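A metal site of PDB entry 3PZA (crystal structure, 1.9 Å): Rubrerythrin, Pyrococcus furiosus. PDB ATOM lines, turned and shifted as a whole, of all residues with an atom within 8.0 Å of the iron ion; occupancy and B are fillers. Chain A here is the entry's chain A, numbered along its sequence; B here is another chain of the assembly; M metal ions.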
ATOM      1  N   TYR A 108       3.506  21.158 -29.833  1.00  0.00           N
ATOM      2  CA  TYR A 108       4.856  21.279 -29.279  1.00  0.00           C
ATOM      3  C   TYR A 108       5.874  20.864 -30.302  1.00  0.00           C
ATOM      4  O   TYR A 108       6.892  21.505 -30.486  1.00  0.00           O
ATOM      5  CB  TYR A 108       4.999  20.346 -28.089  1.00  0.00           C
ATOM      6  CG  TYR A 108       4.320  20.804 -26.816  1.00  0.00           C
ATOM      7  CD1 TYR A 108       3.709  22.091 -26.731  1.00  0.00           C
ATOM      8  CD2 TYR A 108       4.389  19.998 -25.644  1.00  0.00           C
ATOM      9  CE1 TYR A 108       3.134  22.553 -25.506  1.00  0.00           C
ATOM     10  CE2 TYR A 108       3.800  20.474 -24.407  1.00  0.00           C
ATOM     11  CZ  TYR A 108       3.231  21.747 -24.368  1.00  0.00           C
ATOM     12  OH  TYR A 108       2.669  22.204 -23.190  1.00  0.00           O
ATOM     13  N   ILE A 140      17.648  23.241 -24.581  1.00  0.00           N
ATOM     14  CA  ILE A 140      16.415  22.527 -25.029  1.00  0.00           C
ATOM     15  C   ILE A 140      15.380  22.545 -23.948  1.00  0.00           C
ATOM     16  O   ILE A 140      15.680  22.128 -22.802  1.00  0.00           O
ATOM     17  CB  ILE A 140      16.732  21.005 -25.468  1.00  0.00           C
ATOM     18  CG1 ILE A 140      17.885  20.890 -26.433  1.00  0.00           C
ATOM     19  CG2 ILE A 140      15.479  20.369 -26.046  1.00  0.00           C
ATOM     20  CD1 ILE A 140      17.654  21.449 -27.890  1.00  0.00           C
ATOM     21  N   CYS A 141      14.113  22.909 -24.283  1.00  0.00           N
ATOM     22  CA  CYS A 141      13.086  22.808 -23.301  1.00  0.00           C
ATOM     23  C   CYS A 141      12.712  21.305 -23.063  1.00  0.00           C
ATOM     24  O   CYS A 141      12.327  20.634 -23.997  1.00  0.00           O
ATOM     25  CB  CYS A 141      11.873  23.668 -23.708  1.00  0.00           C
ATOM     26  SG  CYS A 141      10.458  23.537 -22.565  1.00  0.00           S
ATOM     27  N   PRO A 142      12.752  20.848 -21.795  1.00  0.00           N
ATOM     28  CA  PRO A 142      12.420  19.444 -21.513  1.00  0.00           C
ATOM     29  C   PRO A 142      10.912  19.172 -21.516  1.00  0.00           C
ATOM     30  O   PRO A 142      10.517  17.993 -21.442  1.00  0.00           O
ATOM     31  CB  PRO A 142      13.060  19.211 -20.133  1.00  0.00           C
ATOM     32  CG  PRO A 142      12.779  20.551 -19.388  1.00  0.00           C
ATOM     33  CD  PRO A 142      13.116  21.581 -20.550  1.00  0.00           C
ATOM     34  N   ILE A 143      10.044  20.191 -21.671  1.00  0.00           N
ATOM     35  CA  ILE A 143       8.604  19.951 -21.769  1.00  0.00           C
ATOM     36  C   ILE A 143       8.134  19.825 -23.250  1.00  0.00           C
ATOM     37  O   ILE A 143       7.385  18.911 -23.609  1.00  0.00           O
ATOM     38  CB  ILE A 143       7.810  21.090 -21.054  1.00  0.00           C
ATOM     39  CG1 ILE A 143       8.272  21.253 -19.558  1.00  0.00           C
ATOM     40  CG2 ILE A 143       6.325  20.944 -21.209  1.00  0.00           C
ATOM     41  CD1 ILE A 143       8.291  20.033 -18.782  1.00  0.00           C
ATOM     42  N   CYS A 144       8.642  20.666 -24.139  1.00  0.00           N
ATOM     43  CA  CYS A 144       8.121  20.695 -25.514  1.00  0.00           C
ATOM     44  C   CYS A 144       9.225  20.630 -26.551  1.00  0.00           C
ATOM     45  O   CYS A 144       8.924  20.547 -27.737  1.00  0.00           O
ATOM     46  CB  CYS A 144       7.277  22.021 -25.722  1.00  0.00           C
ATOM     47  SG  CYS A 144       8.409  23.529 -25.757  1.00  0.00           S
ATOM     48  N   GLY A 145      10.499  20.616 -26.148  1.00  0.00           N
ATOM     49  CA  GLY A 145      11.576  20.504 -27.136  1.00  0.00           C
ATOM     50  C   GLY A 145      11.929  21.781 -27.885  1.00  0.00           C
ATOM     51  O   GLY A 145      12.803  21.813 -28.834  1.00  0.00           O
ATOM     52  N   TYR A 146      11.327  22.892 -27.428  1.00  0.00           N
ATOM     53  CA  TYR A 146      11.782  24.206 -27.943  1.00  0.00           C
ATOM     54  C   TYR A 146      13.331  24.295 -27.896  1.00  0.00           C
ATOM     55  O   TYR A 146      13.903  23.897 -26.863  1.00  0.00           O
ATOM     56  CB  TYR A 146      11.196  25.326 -27.073  1.00  0.00           C
ATOM     57  CG  TYR A 146      11.833  26.663 -27.415  1.00  0.00           C
ATOM     58  CD1 TYR A 146      12.738  27.216 -26.479  1.00  0.00           C
ATOM     59  CD2 TYR A 146      11.539  27.365 -28.649  1.00  0.00           C
ATOM     60  CE1 TYR A 146      13.341  28.467 -26.719  1.00  0.00           C
ATOM     61  CE2 TYR A 146      12.166  28.643 -28.910  1.00  0.00           C
ATOM     62  CZ  TYR A 146      13.063  29.136 -27.881  1.00  0.00           C
ATOM     63  OH  TYR A 146      13.744  30.347 -28.039  1.00  0.00           O
ATOM     64  N   THR A 147      13.993  24.845 -28.923  1.00  0.00           N
ATOM     65  CA  THR A 147      15.481  24.765 -29.051  1.00  0.00           C
ATOM     66  C   THR A 147      15.987  26.181 -29.276  1.00  0.00           C
ATOM     67  O   THR A 147      15.385  26.921 -30.098  1.00  0.00           O
ATOM     68  CB  THR A 147      15.776  23.937 -30.294  1.00  0.00           C
ATOM     69  OG1 THR A 147      15.254  22.603 -30.061  1.00  0.00           O
ATOM     70  CG2 THR A 147      17.278  23.834 -30.625  1.00  0.00           C
ATOM     71  N   TYR A 155      11.580  32.666 -20.642  1.00  0.00           N
ATOM     72  CA  TYR A 155      10.531  31.620 -20.572  1.00  0.00           C
ATOM     73  C   TYR A 155      10.375  30.991 -21.978  1.00  0.00           C
ATOM     74  O   TYR A 155      10.492  31.665 -22.994  1.00  0.00           O
ATOM     75  CB  TYR A 155       9.133  32.206 -20.209  1.00  0.00           C
ATOM     76  CG  TYR A 155       9.218  32.768 -18.807  1.00  0.00           C
ATOM     77  CD1 TYR A 155       9.072  31.934 -17.701  1.00  0.00           C
ATOM     78  CD2 TYR A 155       9.624  34.098 -18.590  1.00  0.00           C
ATOM     79  CE1 TYR A 155       9.261  32.432 -16.437  1.00  0.00           C
ATOM     80  CE2 TYR A 155       9.758  34.611 -17.263  1.00  0.00           C
ATOM     81  CZ  TYR A 155       9.583  33.770 -16.233  1.00  0.00           C
ATOM     82  OH  TYR A 155       9.692  34.264 -14.919  1.00  0.00           O
ATOM     83  N   CYS A 156      10.134  29.685 -22.018  1.00  0.00           N
ATOM     84  CA  CYS A 156       9.890  28.961 -23.298  1.00  0.00           C
ATOM     85  C   CYS A 156       8.715  29.630 -24.011  1.00  0.00           C
ATOM     86  O   CYS A 156       7.654  29.778 -23.377  1.00  0.00           O
ATOM     87  CB  CYS A 156       9.404  27.520 -22.928  1.00  0.00           C
ATOM     88  SG  CYS A 156       9.152  26.649 -24.506  1.00  0.00           S
ATOM     89  N   PRO A 157       8.847  30.044 -25.281  1.00  0.00           N
ATOM     90  CA  PRO A 157       7.658  30.725 -25.931  1.00  0.00           C
ATOM     91  C   PRO A 157       6.482  29.782 -26.258  1.00  0.00           C
ATOM     92  O   PRO A 157       5.310  30.227 -26.511  1.00  0.00           O
ATOM     93  CB  PRO A 157       8.215  31.268 -27.230  1.00  0.00           C
ATOM     94  CG  PRO A 157       9.433  30.337 -27.548  1.00  0.00           C
ATOM     95  CD  PRO A 157       9.988  29.919 -26.180  1.00  0.00           C
ATOM     96  N   VAL A 158       6.739  28.464 -26.159  1.00  0.00           N
ATOM     97  CA  VAL A 158       5.658  27.510 -26.535  1.00  0.00           C
ATOM     98  C   VAL A 158       4.904  27.046 -25.296  1.00  0.00           C
ATOM     99  O   VAL A 158       3.650  27.081 -25.276  1.00  0.00           O
ATOM    100  CB  VAL A 158       6.296  26.267 -27.266  1.00  0.00           C
ATOM    101  CG1 VAL A 158       5.190  25.164 -27.543  1.00  0.00           C
ATOM    102  CG2 VAL A 158       6.985  26.702 -28.512  1.00  0.00           C
ATOM    103  N   CYS A 159       5.589  26.638 -24.234  1.00  0.00           N
ATOM    104  CA  CYS A 159       4.889  26.133 -23.048  1.00  0.00           C
ATOM    105  C   CYS A 159       5.026  27.019 -21.802  1.00  0.00           C
ATOM    106  O   CYS A 159       4.491  26.667 -20.739  1.00  0.00           O
ATOM    107  CB  CYS A 159       5.374  24.726 -22.648  1.00  0.00           C
ATOM    108  SG  CYS A 159       7.095  24.567 -22.082  1.00  0.00           S
ATOM    109  N   GLY A 160       5.892  28.030 -21.895  1.00  0.00           N
ATOM    110  CA  GLY A 160       6.088  28.907 -20.734  1.00  0.00           C
ATOM    111  C   GLY A 160       7.068  28.452 -19.647  1.00  0.00           C
ATOM    112  O   GLY A 160       7.233  29.154 -18.617  1.00  0.00           O
ATOM    113  N   ALA A 161       7.759  27.331 -19.838  1.00  0.00           N
ATOM    114  CA  ALA A 161       8.730  26.799 -18.827  1.00  0.00           C
ATOM    115  C   ALA A 161       9.866  27.816 -18.604  1.00  0.00           C
ATOM    116  O   ALA A 161      10.369  28.412 -19.566  1.00  0.00           O
ATOM    117  CB  ALA A 161       9.386  25.541 -19.316  1.00  0.00           C
ATOM    118  N   PRO A 162      10.312  27.960 -17.341  1.00  0.00           N
ATOM    119  CA  PRO A 162      11.419  28.962 -17.159  1.00  0.00           C
ATOM    120  C   PRO A 162      12.751  28.422 -17.700  1.00  0.00           C
ATOM    121  O   PRO A 162      12.976  27.206 -17.710  1.00  0.00           O
ATOM    122  CB  PRO A 162      11.541  29.100 -15.612  1.00  0.00           C
ATOM    123  CG  PRO A 162      10.739  28.003 -15.035  1.00  0.00           C
ATOM    124  CD  PRO A 162       9.731  27.491 -16.069  1.00  0.00           C
ATOM    125  N   PHE A 166      15.748  24.528 -18.722  1.00  0.00           N
ATOM    126  CA  PHE A 166      16.237  24.069 -19.989  1.00  0.00           C
ATOM    127  C   PHE A 166      17.477  23.213 -19.826  1.00  0.00           C
ATOM    128  O   PHE A 166      18.357  23.522 -19.003  1.00  0.00           O
ATOM    129  CB  PHE A 166      16.605  25.193 -21.011  1.00  0.00           C
ATOM    130  CG  PHE A 166      15.473  26.110 -21.359  1.00  0.00           C
ATOM    131  CD1 PHE A 166      14.156  25.751 -21.098  1.00  0.00           C
ATOM    132  CD2 PHE A 166      15.790  27.393 -21.969  1.00  0.00           C
ATOM    133  CE1 PHE A 166      13.082  26.644 -21.460  1.00  0.00           C
ATOM    134  CE2 PHE A 166      14.774  28.280 -22.336  1.00  0.00           C
ATOM    135  CZ  PHE A 166      13.406  27.924 -22.094  1.00  0.00           C
ATOM    136  N   VAL B  53      12.217  14.471 -26.269  1.00  0.00           N
ATOM    137  CA  VAL B  53      11.123  15.145 -25.628  1.00  0.00           C
ATOM    138  C   VAL B  53       9.844  14.966 -26.459  1.00  0.00           C
ATOM    139  O   VAL B  53       8.755  14.583 -25.887  1.00  0.00           O
ATOM    140  CB  VAL B  53      11.458  16.642 -25.446  1.00  0.00           C
ATOM    141  CG1 VAL B  53      10.195  17.365 -24.824  1.00  0.00           C
ATOM    142  CG2 VAL B  53      12.576  16.797 -24.458  1.00  0.00           C
HETATM  143 FE    FE M   1       8.733  24.542 -23.734  1.00  0.00          FE
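The backbone NH (N) of Cys 156 is in hydrogen-bond range of the backbone carbonyl oxygen (O) of Ala 161.
The side-chain sulfur (SG) of Cys 144 sits close to the backbone NH (N) of Tyr 146, at 3.4 Å.
The side-chain sulfur (SG) of Cys 156 lies close to the backbone NH (N) of Val 158, at 3.4 Å.
The backbone NH (N) of Cys 141 sits at hydrogen-bond distance from the backbone carbonyl oxygen (O) of Tyr 146, at 2.8 Å.
The side-chain sulfur of Cys 141 sits close to the backbone NH of Ile 143.
The side-chain sulfur (SG) of Cys 159 sits close to the backbone NH (N) of Ala 161 (3.6 Å).
Within 4 Å of the iron ion: Cys 141, Cys 144, Cys 156 and Cys 159.
The nearest printed residue that does not touch the iron ion is Tyr 146 (4.2 Å).
The iron ion is bound by SG of Cys 156, 2.3 Å away.
SG of Cys 144 binds the iron ion (2.3 Å).
SG of Cys 141 is bound to the iron ion.
The side-chain sulfur (SG) of Cys 159 is bound to the iron ion, 2.3 Å away.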
